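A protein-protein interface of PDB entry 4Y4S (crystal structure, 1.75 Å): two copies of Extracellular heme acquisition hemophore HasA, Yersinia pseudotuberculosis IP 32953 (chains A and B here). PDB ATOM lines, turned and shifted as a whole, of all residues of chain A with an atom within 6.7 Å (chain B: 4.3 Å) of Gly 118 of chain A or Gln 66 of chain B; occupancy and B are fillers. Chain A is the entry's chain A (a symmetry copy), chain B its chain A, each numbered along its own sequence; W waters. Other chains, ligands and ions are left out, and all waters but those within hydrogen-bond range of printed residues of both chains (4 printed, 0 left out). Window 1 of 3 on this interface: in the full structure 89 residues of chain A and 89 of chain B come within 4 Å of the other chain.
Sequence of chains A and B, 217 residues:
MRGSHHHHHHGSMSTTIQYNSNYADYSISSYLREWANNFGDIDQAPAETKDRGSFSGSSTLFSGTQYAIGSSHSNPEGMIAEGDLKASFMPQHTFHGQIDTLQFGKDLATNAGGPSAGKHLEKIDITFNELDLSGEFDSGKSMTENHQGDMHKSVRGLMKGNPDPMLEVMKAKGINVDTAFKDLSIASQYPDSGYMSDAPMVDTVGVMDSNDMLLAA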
ATOM      1  N   GLY A  64      10.979 -23.241  -4.393  1.00  0.00           N
ATOM      2  CA  GLY A  64      10.895 -24.083  -3.197  1.00  0.00           C
ATOM      3  C   GLY A  64      11.696 -23.467  -2.075  1.00  0.00           C
ATOM      4  O   GLY A  64      12.739 -22.883  -2.343  1.00  0.00           O
ATOM      5  N   THR A  65      11.237 -23.576  -0.832  1.00  0.00           N
ATOM      6  CA  THR A  65      12.029 -23.015   0.258  1.00  0.00           C
ATOM      7  C   THR A  65      12.152 -24.022   1.363  1.00  0.00           C
ATOM      8  O   THR A  65      11.194 -24.757   1.629  1.00  0.00           O
ATOM      9  CB  THR A  65      11.409 -21.755   0.850  1.00  0.00           C
ATOM     10  OG1 THR A  65      10.727 -21.046  -0.185  1.00  0.00           O
ATOM     11  CG2 THR A  65      12.518 -20.839   1.427  1.00  0.00           C
ATOM     12  N   GLN A  66      13.328 -24.047   1.978  1.00  0.00           N
ATOM     13  CA  GLN A  66      13.554 -24.805   3.208  1.00  0.00           C
ATOM     14  C   GLN A  66      14.143 -23.866   4.241  1.00  0.00           C
ATOM     15  O   GLN A  66      15.218 -23.304   4.024  1.00  0.00           O
ATOM     16  CB  GLN A  66      14.490 -25.981   2.992  1.00  0.00           C
ATOM     17  CG  GLN A  66      14.618 -26.888   4.267  1.00  0.00           C
ATOM     18  CD  GLN A  66      15.773 -27.852   4.222  1.00  0.00           C
ATOM     19  OE1 GLN A  66      16.927 -27.425   4.103  1.00  0.00           O
ATOM     20  NE2 GLN A  66      15.493 -29.158   4.332  1.00  0.00           N
ATOM     21  N   TYR A  67      13.448 -23.713   5.362  1.00  0.00           N
ATOM     22  CA  TYR A  67      13.974 -23.016   6.531  1.00  0.00           C
ATOM     23  C   TYR A  67      14.312 -24.001   7.621  1.00  0.00           C
ATOM     24  O   TYR A  67      13.475 -24.810   7.996  1.00  0.00           O
ATOM     25  CB  TYR A  67      12.929 -22.024   7.065  1.00  0.00           C
ATOM     26  CG  TYR A  67      12.475 -20.994   6.072  1.00  0.00           C
ATOM     27  CD1 TYR A  67      13.179 -19.789   5.919  1.00  0.00           C
ATOM     28  CD2 TYR A  67      11.374 -21.202   5.280  1.00  0.00           C
ATOM     29  CE1 TYR A  67      12.764 -18.822   5.001  1.00  0.00           C
ATOM     30  CE2 TYR A  67      10.939 -20.223   4.366  1.00  0.00           C
ATOM     31  CZ  TYR A  67      11.649 -19.055   4.230  1.00  0.00           C
ATOM     32  OH  TYR A  67      11.262 -18.108   3.313  1.00  0.00           O
ATOM     33  N   ALA A  68      15.517 -23.920   8.157  1.00  0.00           N
ATOM     34  CA  ALA A  68      15.919 -24.767   9.272  1.00  0.00           C
ATOM     35  C   ALA A  68      16.325 -23.913  10.473  1.00  0.00           C
ATOM     36  O   ALA A  68      17.078 -22.956  10.319  1.00  0.00           O
ATOM     37  CB  ALA A  68      17.026 -25.619   8.865  1.00  0.00           C
ATOM     38  N   GLU A  82       9.172 -26.244   5.274  1.00  0.00           N
ATOM     39  CA  GLU A  82       9.497 -26.392   3.858  1.00  0.00           C
ATOM     40  C   GLU A  82       8.240 -26.305   3.017  1.00  0.00           C
ATOM     41  O   GLU A  82       7.129 -26.639   3.457  1.00  0.00           O
ATOM     42  CB  GLU A  82      10.204 -27.752   3.664  1.00  0.00           C
ATOM     43  CG  GLU A  82      10.701 -28.056   2.238  1.00  0.00           C
ATOM     44  CD  GLU A  82       9.578 -28.616   1.364  1.00  0.00           C
ATOM     45  OE1 GLU A  82       8.568 -29.111   1.896  1.00  0.00           O
ATOM     46  OE2 GLU A  82       9.716 -28.573   0.130  1.00  0.00           O
ATOM     47  N   ALA A 109      21.418 -31.687  10.165  1.00  0.00           N
ATOM     48  CA  ALA A 109      22.613 -32.161   9.477  1.00  0.00           C
ATOM     49  C   ALA A 109      22.541 -31.837   7.987  1.00  0.00           C
ATOM     50  O   ALA A 109      21.471 -31.609   7.450  1.00  0.00           O
ATOM     51  CB  ALA A 109      22.779 -33.680   9.690  1.00  0.00           C
ATOM     52  N   THR A 110      23.692 -31.788   7.323  1.00  0.00           N
ATOM     53  CA  THR A 110      23.734 -31.425   5.915  1.00  0.00           C
ATOM     54  C   THR A 110      23.361 -32.616   5.103  1.00  0.00           C
ATOM     55  O   THR A 110      23.759 -33.738   5.425  1.00  0.00           O
ATOM     56  CB  THR A 110      25.176 -30.888   5.548  1.00  0.00           C
ATOM     57  OG1 THR A 110      25.440 -29.715   6.302  1.00  0.00           O
ATOM     58  CG2 THR A 110      25.310 -30.522   4.055  1.00  0.00           C
ATOM     59  N   ASN A 111      22.578 -32.403   4.050  1.00  0.00           N
ATOM     60  CA  ASN A 111      22.171 -33.495   3.194  1.00  0.00           C
ATOM     61  C   ASN A 111      23.350 -34.024   2.391  1.00  0.00           C
ATOM     62  O   ASN A 111      24.390 -33.359   2.264  1.00  0.00           O
ATOM     63  CB  ASN A 111      21.030 -33.061   2.256  1.00  0.00           C
ATOM     64  CG  ASN A 111      19.706 -32.891   3.008  1.00  0.00           C
ATOM     65  OD1 ASN A 111      19.430 -33.664   3.908  1.00  0.00           O
ATOM     66  ND2 ASN A 111      18.929 -31.891   2.664  1.00  0.00           N
ATOM     67  N   ALA A 112      23.208 -35.256   1.930  1.00  0.00           N
ATOM     68  CA  ALA A 112      24.116 -35.805   0.934  1.00  0.00           C
ATOM     69  C   ALA A 112      24.147 -34.886  -0.266  1.00  0.00           C
ATOM     70  O   ALA A 112      23.119 -34.415  -0.723  1.00  0.00           O
ATOM     71  CB  ALA A 112      23.662 -37.178   0.517  1.00  0.00           C
ATOM     72  N   GLY A 114      26.110 -32.163  -0.395  1.00  0.00           N
ATOM     73  CA  GLY A 114      26.761 -30.928  -0.057  1.00  0.00           C
ATOM     74  C   GLY A 114      25.880 -29.831   0.472  1.00  0.00           C
ATOM     75  O   GLY A 114      24.660 -29.954   0.594  1.00  0.00           O
ATOM     76  N   PRO A 115      26.509 -28.729   0.813  1.00  0.00           N
ATOM     77  CA  PRO A 115      25.804 -27.618   1.466  1.00  0.00           C
ATOM     78  C   PRO A 115      24.635 -27.108   0.614  1.00  0.00           C
ATOM     79  O   PRO A 115      23.592 -26.751   1.180  1.00  0.00           O
ATOM     80  CB  PRO A 115      26.914 -26.558   1.628  1.00  0.00           C
ATOM     81  CG  PRO A 115      28.186 -27.400   1.702  1.00  0.00           C
ATOM     82  CD  PRO A 115      27.975 -28.541   0.766  1.00  0.00           C
ATOM     83  N   SER A 116      24.792 -27.125  -0.713  1.00  0.00           N
ATOM     84  CA  SER A 116      23.737 -26.685  -1.631  1.00  0.00           C
ATOM     85  C   SER A 116      22.435 -27.455  -1.409  1.00  0.00           C
ATOM     86  O   SER A 116      21.337 -26.909  -1.599  1.00  0.00           O
ATOM     87  CB  SER A 116      24.201 -26.868  -3.076  1.00  0.00           C
ATOM     88  OG  SER A 116      25.087 -25.822  -3.453  1.00  0.00           O
ATOM     89  N   ALA A 117      22.568 -28.717  -0.994  1.00  0.00           N
ATOM     90  CA  ALA A 117      21.403 -29.621  -0.847  1.00  0.00           C
ATOM     91  C   ALA A 117      20.568 -29.418   0.436  1.00  0.00           C
ATOM     92  O   ALA A 117      19.592 -30.126   0.672  1.00  0.00           O
ATOM     93  CB  ALA A 117      21.899 -31.091  -0.934  1.00  0.00           C
ATOM     94  N   GLY A 118      20.935 -28.456   1.259  1.00  0.00           N
ATOM     95  CA  GLY A 118      20.132 -28.124   2.426  1.00  0.00           C
ATOM     96  C   GLY A 118      20.328 -29.121   3.569  1.00  0.00           C
ATOM     97  O   GLY A 118      21.337 -29.863   3.628  1.00  0.00           O
ATOM     98  N   LYS A 119      19.329 -29.154   4.455  1.00  0.00           N
ATOM     99  CA  LYS A 119      19.430 -29.849   5.734  1.00  0.00           C
ATOM    100  C   LYS A 119      18.431 -30.992   5.898  1.00  0.00           C
ATOM    101  O   LYS A 119      17.449 -31.046   5.184  1.00  0.00           O
ATOM    102  CB  LYS A 119      19.210 -28.827   6.853  1.00  0.00           C
ATOM    103  CG  LYS A 119      20.141 -27.604   6.836  1.00  0.00           C
ATOM    104  CD  LYS A 119      21.609 -28.014   7.036  1.00  0.00           C
ATOM    105  CE  LYS A 119      22.535 -26.791   7.311  1.00  0.00           C
ATOM    106  NZ  LYS A 119      22.675 -25.934   6.050  1.00  0.00           N
ATOM    107  N   HIS A 120      18.680 -31.901   6.843  1.00  0.00           N
ATOM    108  CA  HIS A 120      17.628 -32.820   7.308  1.00  0.00           C
ATOM    109  C   HIS A 120      17.779 -32.933   8.810  1.00  0.00           C
ATOM    110  O   HIS A 120      18.804 -32.571   9.336  1.00  0.00           O
ATOM    111  CB  HIS A 120      17.715 -34.217   6.689  1.00  0.00           C
ATOM    112  CG  HIS A 120      19.008 -34.915   6.997  1.00  0.00           C
ATOM    113  ND1 HIS A 120      20.128 -34.776   6.217  1.00  0.00           N
ATOM    114  CD2 HIS A 120      19.356 -35.742   8.014  1.00  0.00           C
ATOM    115  CE1 HIS A 120      21.125 -35.483   6.740  1.00  0.00           C
ATOM    116  NE2 HIS A 120      20.678 -36.080   7.829  1.00  0.00           N
ATOM    117  N   THR B  65      18.979 -21.598   5.258  1.00  0.00           N
ATOM    118  CA  THR B  65      17.935 -21.432   4.251  1.00  0.00           C
ATOM    119  C   THR B  65      18.375 -22.055   2.959  1.00  0.00           C
ATOM    120  O   THR B  65      19.562 -21.981   2.618  1.00  0.00           O
ATOM    121  CB  THR B  65      17.615 -19.969   3.969  1.00  0.00           C
ATOM    122  OG1 THR B  65      17.794 -19.217   5.171  1.00  0.00           O
ATOM    123  CG2 THR B  65      16.140 -19.826   3.513  1.00  0.00           C
ATOM    124  N   GLN B  66      17.419 -22.668   2.272  1.00  0.00           N
ATOM    125  CA  GLN B  66      17.618 -23.139   0.901  1.00  0.00           C
ATOM    126  C   GLN B  66      16.509 -22.571   0.041  1.00  0.00           C
ATOM    127  O   GLN B  66      15.332 -22.838   0.291  1.00  0.00           O
ATOM    128  CB  GLN B  66      17.611 -24.655   0.810  1.00  0.00           C
ATOM    129  CG  GLN B  66      17.975 -25.171  -0.627  1.00  0.00           C
ATOM    130  CD  GLN B  66      17.653 -26.623  -0.858  1.00  0.00           C
ATOM    131  OE1 GLN B  66      16.490 -27.024  -0.736  1.00  0.00           O
ATOM    132  NE2 GLN B  66      18.663 -27.431  -1.209  1.00  0.00           N
ATOM    133  N   TYR B  67      16.886 -21.803  -0.975  1.00  0.00           N
ATOM    134  CA  TYR B  67      15.964 -21.354  -2.014  1.00  0.00           C
ATOM    135  C   TYR B  67      16.222 -22.096  -3.300  1.00  0.00           C
ATOM    136  O   TYR B  67      17.350 -22.129  -3.771  1.00  0.00           O
ATOM    137  CB  TYR B  67      16.147 -19.849  -2.262  1.00  0.00           C
ATOM    138  CG  TYR B  67      15.946 -18.982  -1.053  1.00  0.00           C
ATOM    139  CD1 TYR B  67      14.667 -18.519  -0.710  1.00  0.00           C
ATOM    140  CD2 TYR B  67      16.997 -18.630  -0.245  1.00  0.00           C
ATOM    141  CE1 TYR B  67      14.468 -17.710   0.411  1.00  0.00           C
ATOM    142  CE2 TYR B  67      16.807 -17.799   0.877  1.00  0.00           C
ATOM    143  CZ  TYR B  67      15.544 -17.364   1.195  1.00  0.00           C
ATOM    144  OH  TYR B  67      15.336 -16.587   2.309  1.00  0.00           O
ATOM    145  N   ALA B  68      15.184 -22.660  -3.892  1.00  0.00           N
ATOM    146  CA  ALA B  68      15.305 -23.329  -5.179  1.00  0.00           C
ATOM    147  C   ALA B  68      14.381 -22.681  -6.209  1.00  0.00           C
ATOM    148  O   ALA B  68      13.214 -22.437  -5.919  1.00  0.00           O
ATOM    149  CB  ALA B  68      14.979 -24.740  -5.031  1.00  0.00           C
ATOM    150  N   ILE B  80      19.956 -23.089  -7.133  1.00  0.00           N
ATOM    151  CA  ILE B  80      19.804 -23.183  -5.682  1.00  0.00           C
ATOM    152  C   ILE B  80      20.697 -22.157  -5.011  1.00  0.00           C
ATOM    153  O   ILE B  80      21.913 -22.104  -5.290  1.00  0.00           O
ATOM    154  CB  ILE B  80      20.177 -24.613  -5.222  1.00  0.00           C
ATOM    155  CG1 ILE B  80      19.195 -25.618  -5.796  1.00  0.00           C
ATOM    156  CG2 ILE B  80      20.165 -24.729  -3.684  1.00  0.00           C
ATOM    157  CD1 ILE B  80      19.491 -26.998  -5.308  1.00  0.00           C
ATOM    158  N   ALA B  81      20.097 -21.325  -4.156  1.00  0.00           N
ATOM    159  CA  ALA B  81      20.861 -20.489  -3.262  1.00  0.00           C
ATOM    160  C   ALA B  81      20.710 -20.998  -1.814  1.00  0.00           C
ATOM    161  O   ALA B  81      19.599 -21.216  -1.334  1.00  0.00           O
ATOM    162  CB  ALA B  81      20.400 -19.000  -3.387  1.00  0.00           C
ATOM    163  N   GLY B 118      14.153 -30.831   1.556  1.00  0.00           N
ATOM    164  CA  GLY B 118      14.503 -29.852   0.539  1.00  0.00           C
ATOM    165  C   GLY B 118      14.877 -30.505  -0.793  1.00  0.00           C
ATOM    166  O   GLY B 118      14.529 -31.677  -1.071  1.00  0.00           O
ATOM    167  N   LYS B 119      15.624 -29.742  -1.595  1.00  0.00           N
ATOM    168  CA  LYS B 119      15.879 -30.079  -2.993  1.00  0.00           C
ATOM    169  C   LYS B 119      17.353 -30.313  -3.313  1.00  0.00           C
ATOM    170  O   LYS B 119      18.211 -29.899  -2.558  1.00  0.00           O
ATOM    171  CB  LYS B 119      15.351 -28.936  -3.864  1.00  0.00           C
ATOM    172  CG  LYS B 119      13.871 -28.570  -3.666  1.00  0.00           C
ATOM    173  CD  LYS B 119      12.949 -29.739  -4.046  1.00  0.00           C
ATOM    174  CE  LYS B 119      11.453 -29.311  -4.133  1.00  0.00           C
ATOM    175  NZ  LYS B 119      10.908 -28.994  -2.737  1.00  0.00           N
HETATM  176  O   HOH W   1      11.565 -31.054  -0.892  1.00  0.00           O
HETATM  177  O   HOH W   2      11.961 -26.907  -1.317  1.00  0.00           O
HETATM  178  O   HOH W   3      14.267 -25.554  -1.121  1.00  0.00           O
HETATM  179  O   HOH W   4      20.472 -24.691   5.010  1.00  0.00           O
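Thr 65 of chain A touches Gln 66 of chain B, and with the chains exchanged Gln 66 of chain A touches Thr 65 of chain B. Thr 65 of chain A touches Tyr 67 of chain B, and with the chains exchanged Tyr 67 of chain A touches Thr 65 of chain B. Gln 66 of chain A touches its own counterpart, Gln 66 of chain B. Gln 66 of chain A touches Gly 118 of chain B, and with the chains exchanged Gly 118 of chain A touches Gln 66 of chain B.
Hydrophobic or aromatic side chains of chain A that line the printed part of chain B: Tyr 67. Of the 8 printed residues of chain B, 7 touch a printed residue of chain A. Hydrophobic or aromatic side chains of chain B that line the printed part of chain A: Tyr 67, Ala 68 and Ile 80. Among the printed residues, Asp or Glu carboxylates within 4 Å of a Lys or Arg side-chain nitrogen of the other chain: Glu 82 of chain A with Lys 119 of chain B.
Among the printed residues, pairs that only touch across the chains: Gly 64 of chain A with Gln 66 of chain B, Gly 64 of chain A with Tyr 67 of chain B, Thr 65 of chain A with Gln 66 of chain B, Thr 65 of chain A with Tyr 67 of chain B, Gln 66 of chain A with Thr 65 of chain B, Gln 66 of chain A with Gly 118 of chain B, Tyr 67 of chain A with Thr 65 of chain B, Ser 116 of chain A with Ile 80 of chain B, Ala 117 of chain A with Lys 119 of chain B and Gly 118 of chain A with Gln 66 of chain B.
NE2 of Gln 66 of chain B sits at hydrogen-bond distance from O of Lys 119 of chain B (2.8 Å). N of Tyr 67 of chain B is in hydrogen-bond range of O of Ala 81 of chain B, at 2.8 Å. The backbone carbonyl oxygen (O) of Lys 119 of chain A lies within hydrogen-bond range of the side-chain amide nitrogen (NE2) of Gln 66 of chain A (2.8 Å). The side-chain amide nitrogen (ND2) of Asn 111 of chain A lies within hydrogen-bond range of the backbone carbonyl oxygen (O) of Ala 117 of chain A (2.7 Å). O of Gly 118 of chain A is in hydrogen-bond range of N of Asn 111 of chain A.
Of the printed residues of chain B, Gly 64 of chain A touches Gln 66, Tyr 67 and Ala 68. Of the printed residues of chain B, Gln 66 of chain A touches Thr 65, Gln 66 and Gly 118. Printed residues of chain A within 4 Å of Gln 66 of chain B: Gly 64, Thr 65, Gln 66, Ser 116, Ala 117 and Gly 118. Printed residues of chain A within 4 Å of Tyr 67 of chain B: Gly 64 and Thr 65. Of the printed residues of chain A, Lys 119 of chain B touches Glu 82 (3.1 Å) and Ala 117 (3.5 Å). The nearest printed residue of chain B that does not touch Gly 118 of chain A is Lys 119 of chain B (4.9 Å).
The backbone NH of Gln 66 of chain B is in hydrogen-bond range of the backbone carbonyl oxygen of Gln 66 of chain A (2.9 Å). The backbone carbonyl oxygen (O) of Ser 116 of chain A is in hydrogen-bond range of the side-chain amide nitrogen (NE2) of Gln 66 of chain B, 2.8 Å away. The side-chain amide nitrogen of Gln 66 of chain B lies close to the backbone carbonyl oxygen of Ala 117 of chain A (3.4 Å). The backbone carbonyl oxygen of Ala 68 of chain B lies within hydrogen-bond range of the backbone NH of Gly 64 of chain A. The side-chain amino group (NZ) of Lys 119 of chain B is in salt-bridge range of the side-chain carboxylate (OE2) of Glu 82 of chain A, at 3.1 Å.
Water W3 bridges OE1 of Gln 66 of chain B (2.7 Å) and O of Gly 64 of chain A (3.3 Å). Water W2 lies within hydrogen-bond range of the side-chain amino group of Lys 119 of chain B, the side-chain carboxylate of Glu 82 of chain A and the backbone NH of Thr 65 of chain A. Water W4 bridges the side-chain amino group of Lys 119 of chain A and the backbone NH of Thr 65 of chain B. Water W1 lies within hydrogen-bond range of the side-chain amino group of Lys 119 of chain B (2.8 Å), the backbone carbonyl oxygen of Gly 118 of chain B (3.0 Å) and the side-chain carboxylate of Glu 82 of chain A (3.3 Å).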
